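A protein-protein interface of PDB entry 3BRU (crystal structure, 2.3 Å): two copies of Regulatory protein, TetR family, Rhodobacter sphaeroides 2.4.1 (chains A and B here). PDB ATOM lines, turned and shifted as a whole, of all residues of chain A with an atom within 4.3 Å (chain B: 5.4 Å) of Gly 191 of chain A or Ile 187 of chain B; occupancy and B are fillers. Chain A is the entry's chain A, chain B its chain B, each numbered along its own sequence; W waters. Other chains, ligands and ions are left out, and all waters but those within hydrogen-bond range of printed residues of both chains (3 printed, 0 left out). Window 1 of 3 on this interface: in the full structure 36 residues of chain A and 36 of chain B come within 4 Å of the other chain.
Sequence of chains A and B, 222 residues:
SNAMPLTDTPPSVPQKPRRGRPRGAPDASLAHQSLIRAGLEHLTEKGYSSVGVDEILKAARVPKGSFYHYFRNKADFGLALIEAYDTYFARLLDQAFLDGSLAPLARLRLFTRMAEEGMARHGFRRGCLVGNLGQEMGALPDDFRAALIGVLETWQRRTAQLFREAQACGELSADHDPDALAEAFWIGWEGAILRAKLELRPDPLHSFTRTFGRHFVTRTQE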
ATOM      1  N   ILE A 187      15.138   7.757 -19.648  1.00  0.00           N
ATOM      2  CA  ILE A 187      15.487   8.827 -20.608  1.00  0.00           C
ATOM      3  C   ILE A 187      15.365   8.275 -22.054  1.00  0.00           C
ATOM      4  O   ILE A 187      14.695   8.855 -22.900  1.00  0.00           O
ATOM      5  CB  ILE A 187      16.947   9.378 -20.412  1.00  0.00           C
ATOM      6  CG1 ILE A 187      17.113  10.203 -19.124  1.00  0.00           C
ATOM      7  CG2 ILE A 187      17.425  10.127 -21.682  1.00  0.00           C
ATOM      8  CD1 ILE A 187      18.579  10.537 -18.781  1.00  0.00           C
ATOM      9  N   GLY A 188      16.005   7.148 -22.320  1.00  0.00           N
ATOM     10  CA  GLY A 188      16.045   6.608 -23.673  1.00  0.00           C
ATOM     11  C   GLY A 188      14.733   6.043 -24.163  1.00  0.00           C
ATOM     12  O   GLY A 188      14.357   6.244 -25.335  1.00  0.00           O
ATOM     13  N   TRP A 189      14.024   5.355 -23.268  1.00  0.00           N
ATOM     14  CA  TRP A 189      12.707   4.763 -23.603  1.00  0.00           C
ATOM     15  C   TRP A 189      11.617   5.774 -23.945  1.00  0.00           C
ATOM     16  O   TRP A 189      10.835   5.566 -24.822  1.00  0.00           O
ATOM     17  CB  TRP A 189      12.263   3.854 -22.469  1.00  0.00           C
ATOM     18  CG  TRP A 189      10.985   3.170 -22.681  1.00  0.00           C
ATOM     19  CD1 TRP A 189       9.838   3.379 -21.991  1.00  0.00           C
ATOM     20  CD2 TRP A 189      10.704   2.156 -23.646  1.00  0.00           C
ATOM     21  NE1 TRP A 189       8.843   2.542 -22.454  1.00  0.00           N
ATOM     22  CE2 TRP A 189       9.349   1.786 -23.479  1.00  0.00           C
ATOM     23  CE3 TRP A 189      11.453   1.543 -24.665  1.00  0.00           C
ATOM     24  CZ2 TRP A 189       8.729   0.801 -24.276  1.00  0.00           C
ATOM     25  CZ3 TRP A 189      10.837   0.562 -25.459  1.00  0.00           C
ATOM     26  CH2 TRP A 189       9.486   0.207 -25.256  1.00  0.00           C
ATOM     27  N   GLU A 190      11.575   6.884 -23.232  1.00  0.00           N
ATOM     28  CA  GLU A 190      10.661   7.972 -23.587  1.00  0.00           C
ATOM     29  C   GLU A 190      10.983   8.591 -24.965  1.00  0.00           C
ATOM     30  O   GLU A 190      10.065   9.028 -25.686  1.00  0.00           O
ATOM     31  CB  GLU A 190      10.649   9.054 -22.492  1.00  0.00           C
ATOM     32  CG  GLU A 190       9.917   8.672 -21.214  1.00  0.00           C
ATOM     33  CD  GLU A 190       8.390   8.479 -21.390  1.00  0.00           C
ATOM     34  OE1 GLU A 190       7.780   9.015 -22.362  1.00  0.00           O
ATOM     35  OE2 GLU A 190       7.788   7.769 -20.551  1.00  0.00           O
ATOM     36  N   GLY A 191      12.271   8.623 -25.325  1.00  0.00           N
ATOM     37  CA  GLY A 191      12.704   9.165 -26.608  1.00  0.00           C
ATOM     38  C   GLY A 191      12.437   8.197 -27.735  1.00  0.00           C
ATOM     39  O   GLY A 191      12.178   8.614 -28.877  1.00  0.00           O
ATOM     40  N   ALA A 192      12.536   6.891 -27.434  1.00  0.00           N
ATOM     41  CA  ALA A 192      12.140   5.826 -28.377  1.00  0.00           C
ATOM     42  C   ALA A 192      10.616   5.875 -28.669  1.00  0.00           C
ATOM     43  O   ALA A 192      10.197   5.778 -29.816  1.00  0.00           O
ATOM     44  CB  ALA A 192      12.570   4.459 -27.859  1.00  0.00           C
ATOM     45  N   ILE A 193       9.803   6.051 -27.626  1.00  0.00           N
ATOM     46  CA  ILE A 193       8.365   6.239 -27.798  1.00  0.00           C
ATOM     47  C   ILE A 193       8.029   7.478 -28.625  1.00  0.00           C
ATOM     48  O   ILE A 193       7.197   7.403 -29.533  1.00  0.00           O
ATOM     49  CB  ILE A 193       7.611   6.238 -26.477  1.00  0.00           C
ATOM     50  CG1 ILE A 193       7.512   4.815 -25.943  1.00  0.00           C
ATOM     51  CG2 ILE A 193       6.171   6.768 -26.669  1.00  0.00           C
ATOM     52  CD1 ILE A 193       7.402   4.809 -24.444  1.00  0.00           C
ATOM     53  N   LEU A 194       8.674   8.603 -28.322  1.00  0.00           N
ATOM     54  CA  LEU A 194       8.546   9.789 -29.129  1.00  0.00           C
ATOM     55  C   LEU A 194       8.694   9.466 -30.606  1.00  0.00           C
ATOM     56  O   LEU A 194       7.830   9.853 -31.429  1.00  0.00           O
ATOM     57  CB  LEU A 194       9.585  10.828 -28.698  1.00  0.00           C
ATOM     58  CG  LEU A 194       9.553  12.224 -29.316  1.00  0.00           C
ATOM     59  CD1 LEU A 194      10.285  13.286 -28.361  1.00  0.00           C
ATOM     60  CD2 LEU A 194      10.081  12.303 -30.783  1.00  0.00           C
ATOM     61  N   ARG A 195       9.782   8.747 -30.920  1.00  0.00           N
ATOM     62  CA  ARG A 195      10.186   8.405 -32.280  1.00  0.00           C
ATOM     63  C   ARG A 195       9.290   7.364 -32.950  1.00  0.00           C
ATOM     64  O   ARG A 195       9.064   7.442 -34.161  1.00  0.00           O
ATOM     65  CB  ARG A 195      11.656   7.969 -32.309  1.00  0.00           C
ATOM     66  CG  ARG A 195      12.674   9.137 -32.202  1.00  0.00           C
ATOM     67  CD  ARG A 195      12.727  10.008 -33.455  1.00  0.00           C
ATOM     68  NE  ARG A 195      13.301   9.293 -34.590  1.00  0.00           N
ATOM     69  CZ  ARG A 195      14.601   9.177 -34.841  1.00  0.00           C
ATOM     70  NH1 ARG A 195      15.504   9.744 -34.031  1.00  0.00           N
ATOM     71  NH2 ARG A 195      14.993   8.469 -35.902  1.00  0.00           N
ATOM     72  N   PRO A 204      12.100   2.388 -33.883  1.00  0.00           N
ATOM     73  CA  PRO A 204      12.900   3.090 -32.862  1.00  0.00           C
ATOM     74  C   PRO A 204      12.907   2.394 -31.504  1.00  0.00           C
ATOM     75  O   PRO A 204      13.875   2.554 -30.751  1.00  0.00           O
ATOM     76  CB  PRO A 204      12.225   4.462 -32.761  1.00  0.00           C
ATOM     77  CG  PRO A 204      11.450   4.606 -34.035  1.00  0.00           C
ATOM     78  CD  PRO A 204      10.978   3.234 -34.352  1.00  0.00           C
ATOM     79  N   PHE A 208      16.441   1.273 -29.988  1.00  0.00           N
ATOM     80  CA  PHE A 208      16.809   1.630 -28.622  1.00  0.00           C
ATOM     81  C   PHE A 208      17.186   0.414 -27.722  1.00  0.00           C
ATOM     82  O   PHE A 208      18.215   0.432 -27.058  1.00  0.00           O
ATOM     83  CB  PHE A 208      15.742   2.502 -27.933  1.00  0.00           C
ATOM     84  CG  PHE A 208      15.919   2.553 -26.436  1.00  0.00           C
ATOM     85  CD1 PHE A 208      16.987   3.267 -25.873  1.00  0.00           C
ATOM     86  CD2 PHE A 208      15.082   1.810 -25.600  1.00  0.00           C
ATOM     87  CE1 PHE A 208      17.202   3.277 -24.507  1.00  0.00           C
ATOM     88  CE2 PHE A 208      15.294   1.811 -24.207  1.00  0.00           C
ATOM     89  CZ  PHE A 208      16.356   2.564 -23.661  1.00  0.00           C
ATOM     90  N   GLN B 156      21.601  11.781 -37.966  1.00  0.00           N
ATOM     91  CA  GLN B 156      22.042  10.409 -37.726  1.00  0.00           C
ATOM     92  C   GLN B 156      23.125  10.010 -38.741  1.00  0.00           C
ATOM     93  O   GLN B 156      24.108   9.391 -38.356  1.00  0.00           O
ATOM     94  CB  GLN B 156      20.846   9.424 -37.744  1.00  0.00           C
ATOM     95  CG  GLN B 156      19.911   9.494 -36.497  1.00  0.00           C
ATOM     96  CD  GLN B 156      18.583   8.735 -36.643  1.00  0.00           C
ATOM     97  OE1 GLN B 156      17.753   8.779 -35.748  1.00  0.00           O
ATOM     98  NE2 GLN B 156      18.373   8.067 -37.774  1.00  0.00           N
ATOM     99  N   ALA B 182      24.252   5.398 -34.040  1.00  0.00           N
ATOM    100  CA  ALA B 182      23.893   6.780 -34.314  1.00  0.00           C
ATOM    101  C   ALA B 182      22.398   6.993 -34.068  1.00  0.00           C
ATOM    102  O   ALA B 182      21.973   8.047 -33.567  1.00  0.00           O
ATOM    103  CB  ALA B 182      24.248   7.149 -35.706  1.00  0.00           C
ATOM    104  N   GLU B 183      21.597   5.996 -34.409  1.00  0.00           N
ATOM    105  CA  GLU B 183      20.180   6.140 -34.201  1.00  0.00           C
ATOM    106  C   GLU B 183      19.892   6.156 -32.696  1.00  0.00           C
ATOM    107  O   GLU B 183      19.146   7.044 -32.227  1.00  0.00           O
ATOM    108  CB  GLU B 183      19.342   5.080 -34.925  1.00  0.00           C
ATOM    109  CG  GLU B 183      17.886   5.211 -34.441  1.00  0.00           C
ATOM    110  CD  GLU B 183      16.800   4.602 -35.331  1.00  0.00           C
ATOM    111  OE1 GLU B 183      17.143   3.913 -36.306  1.00  0.00           O
ATOM    112  OE2 GLU B 183      15.587   4.806 -35.027  1.00  0.00           O
ATOM    113  N   ALA B 184      20.467   5.192 -31.950  1.00  0.00           N
ATOM    114  CA  ALA B 184      20.362   5.181 -30.494  1.00  0.00           C
ATOM    115  C   ALA B 184      20.858   6.485 -29.858  1.00  0.00           C
ATOM    116  O   ALA B 184      20.276   6.922 -28.865  1.00  0.00           O
ATOM    117  CB  ALA B 184      21.090   4.023 -29.909  1.00  0.00           C
ATOM    118  N   PHE B 185      21.944   7.091 -30.377  1.00  0.00           N
ATOM    119  CA  PHE B 185      22.425   8.352 -29.790  1.00  0.00           C
ATOM    120  C   PHE B 185      21.330   9.435 -29.866  1.00  0.00           C
ATOM    121  O   PHE B 185      21.040  10.090 -28.874  1.00  0.00           O
ATOM    122  CB  PHE B 185      23.737   8.854 -30.405  1.00  0.00           C
ATOM    123  CG  PHE B 185      24.154  10.224 -29.874  1.00  0.00           C
ATOM    124  CD1 PHE B 185      24.860  10.334 -28.672  1.00  0.00           C
ATOM    125  CD2 PHE B 185      23.740  11.395 -30.514  1.00  0.00           C
ATOM    126  CE1 PHE B 185      25.189  11.550 -28.139  1.00  0.00           C
ATOM    127  CE2 PHE B 185      24.043  12.642 -29.982  1.00  0.00           C
ATOM    128  CZ  PHE B 185      24.788  12.732 -28.792  1.00  0.00           C
ATOM    129  N   TRP B 186      20.697   9.592 -31.030  1.00  0.00           N
ATOM    130  CA  TRP B 186      19.694  10.634 -31.222  1.00  0.00           C
ATOM    131  C   TRP B 186      18.395  10.359 -30.499  1.00  0.00           C
ATOM    132  O   TRP B 186      17.784  11.288 -29.980  1.00  0.00           O
ATOM    133  CB  TRP B 186      19.501  10.950 -32.716  1.00  0.00           C
ATOM    134  CG  TRP B 186      20.690  11.772 -33.141  1.00  0.00           C
ATOM    135  CD1 TRP B 186      21.815  11.325 -33.763  1.00  0.00           C
ATOM    136  CD2 TRP B 186      20.911  13.163 -32.855  1.00  0.00           C
ATOM    137  NE1 TRP B 186      22.714  12.360 -33.908  1.00  0.00           N
ATOM    138  CE2 TRP B 186      22.185  13.493 -33.358  1.00  0.00           C
ATOM    139  CE3 TRP B 186      20.134  14.170 -32.228  1.00  0.00           C
ATOM    140  CZ2 TRP B 186      22.714  14.777 -33.270  1.00  0.00           C
ATOM    141  CZ3 TRP B 186      20.648  15.431 -32.130  1.00  0.00           C
ATOM    142  CH2 TRP B 186      21.938  15.737 -32.651  1.00  0.00           C
ATOM    143  N   ILE B 187      17.982   9.086 -30.441  1.00  0.00           N
ATOM    144  CA  ILE B 187      16.844   8.696 -29.644  1.00  0.00           C
ATOM    145  C   ILE B 187      17.029   9.137 -28.186  1.00  0.00           C
ATOM    146  O   ILE B 187      16.138   9.763 -27.595  1.00  0.00           O
ATOM    147  CB  ILE B 187      16.627   7.194 -29.699  1.00  0.00           C
ATOM    148  CG1 ILE B 187      15.986   6.806 -31.025  1.00  0.00           C
ATOM    149  CG2 ILE B 187      15.744   6.701 -28.502  1.00  0.00           C
ATOM    150  CD1 ILE B 187      16.095   5.306 -31.312  1.00  0.00           C
ATOM    151  N   GLY B 188      18.173   8.790 -27.605  1.00  0.00           N
ATOM    152  CA  GLY B 188      18.411   9.080 -26.196  1.00  0.00           C
ATOM    153  C   GLY B 188      18.703  10.546 -25.916  1.00  0.00           C
ATOM    154  O   GLY B 188      18.297  11.057 -24.867  1.00  0.00           O
ATOM    155  N   TRP B 189      19.402  11.219 -26.838  1.00  0.00           N
ATOM    156  CA  TRP B 189      19.771  12.629 -26.668  1.00  0.00           C
ATOM    157  C   TRP B 189      18.539  13.538 -26.639  1.00  0.00           C
ATOM    158  O   TRP B 189      18.425  14.385 -25.756  1.00  0.00           O
ATOM    159  CB  TRP B 189      20.792  13.067 -27.722  1.00  0.00           C
ATOM    160  CG  TRP B 189      21.240  14.489 -27.587  1.00  0.00           C
ATOM    161  CD1 TRP B 189      21.009  15.503 -28.477  1.00  0.00           C
ATOM    162  CD2 TRP B 189      21.963  15.083 -26.483  1.00  0.00           C
ATOM    163  NE1 TRP B 189      21.564  16.674 -28.014  1.00  0.00           N
ATOM    164  CE2 TRP B 189      22.148  16.453 -26.797  1.00  0.00           C
ATOM    165  CE3 TRP B 189      22.469  14.588 -25.261  1.00  0.00           C
ATOM    166  CZ2 TRP B 189      22.815  17.352 -25.932  1.00  0.00           C
ATOM    167  CZ3 TRP B 189      23.139  15.474 -24.391  1.00  0.00           C
ATOM    168  CH2 TRP B 189      23.308  16.848 -24.739  1.00  0.00           C
ATOM    169  N   GLU B 190      17.593  13.337 -27.560  1.00  0.00           N
ATOM    170  CA  GLU B 190      16.309  14.039 -27.489  1.00  0.00           C
ATOM    171  C   GLU B 190      15.524  13.735 -26.188  1.00  0.00           C
ATOM    172  O   GLU B 190      14.916  14.647 -25.570  1.00  0.00           O
ATOM    173  CB  GLU B 190      15.452  13.702 -28.716  1.00  0.00           C
ATOM    174  CG  GLU B 190      16.048  14.255 -30.014  1.00  0.00           C
ATOM    175  CD  GLU B 190      15.836  15.778 -30.142  1.00  0.00           C
ATOM    176  OE1 GLU B 190      15.122  16.389 -29.278  1.00  0.00           O
ATOM    177  OE2 GLU B 190      16.369  16.366 -31.117  1.00  0.00           O
ATOM    178  N   GLY B 191      15.533  12.471 -25.774  1.00  0.00           N
ATOM    179  CA  GLY B 191      15.014  12.093 -24.442  1.00  0.00           C
ATOM    180  C   GLY B 191      15.673  12.824 -23.269  1.00  0.00           C
ATOM    181  O   GLY B 191      15.004  13.174 -22.299  1.00  0.00           O
HETATM  182  O   HOH W   1      13.045  11.264 -21.892  1.00  0.00           O
HETATM  183  O   HOH W   2      13.902  10.585 -29.358  1.00  0.00           O
HETATM  184  O   HOH W   3      15.210  11.268 -31.663  1.00  0.00           O
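The guanidinium group of Arg 195 of chain A lies within hydrogen-bond range of the side-chain amide oxygen of Gln 156 of chain B, at 2.8 Å.
NH2 of Arg 195 of chain A lies within salt-bridge range of OE2 of Glu 183 of chain B (3.8 Å).
Gly 188 of chain B touches Ile 187 of chain A.
Ile 187 of chain A touches Gly 191 of chain B.
Gly 188 of chain A touches Ile 187 of chain B.
Ile 187 of chain B touches Gly 191 of chain A (O to CA, 3.6 Å).
Ile 187 of chain B touches Ala 192 of chain A (CG2 to N, 3.4 Å).
Glu 183 of chain B touches Pro 204 of chain A.
O of Pro 204 of chain A touches CD1 of Ile 187 of chain B (3.6 Å).
Of chain B, only Ile 187 (3.6 Å) comes within 4 Å of Gly 191 of chain A.
Of the printed residues of chain B, Ala 192 of chain A touches Ile 187.
Leu 194 of chain A touches none of the printed residues of chain B.
Printed residues of chain B within 4 Å of Arg 195 of chain A: Gln 156 and Glu 183.
Printed residues of chain A within 4 Å of Glu 183 of chain B: Arg 195 and Pro 204.
Of the printed residues of chain A, Ile 187 of chain B touches Gly 188 (3.5 Å), Gly 191 (3.6 Å), Ala 192 (3.4 Å) and Pro 204 (3.6 Å).
The nearest printed residue of chain A that does not touch Glu 183 of chain B is Phe 208 of chain A (6.1 Å).
Of the 11 printed residues of chain B, 5 touch a printed residue of chain A.
Printed residues of chain B that touch a printed residue of chain A: Gln 156, Glu 183, Ile 187, Gly 188 and Gly 191.
Hydrophobic or aromatic side chains of chain B within 4 Å of the printed part of chain A: Ile 187.
Among the printed residues, Asp or Glu carboxylates within 4 Å of a Lys or Arg side-chain nitrogen of the other chain: Arg 195 of chain A with Glu 183 of chain B (3.8 Å).
Ile 187 of chain A touches Gly 188 of chain B, and with the chains exchanged Gly 188 of chain A touches Ile 187 of chain B.
Ile 187 of chain A touches Gly 191 of chain B, and with the chains exchanged Gly 191 of chain A touches Ile 187 of chain B.
Water W2 lies within hydrogen-bond range of the backbone carbonyl oxygen (O) of Gly 191 of chain A (2.7 Å) and the backbone carbonyl oxygen (O) of Ile 187 of chain B (3.0 Å).
Water W1 bridges the backbone carbonyl oxygen (O) of Gly 191 of chain B and the backbone carbonyl oxygen (O) of Ile 187 of chain A.
Water W3 lies within hydrogen-bond range of NH1 of Arg 195 of chain A (2.8 Å) and O of Trp 186 of chain B (3.1 Å).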
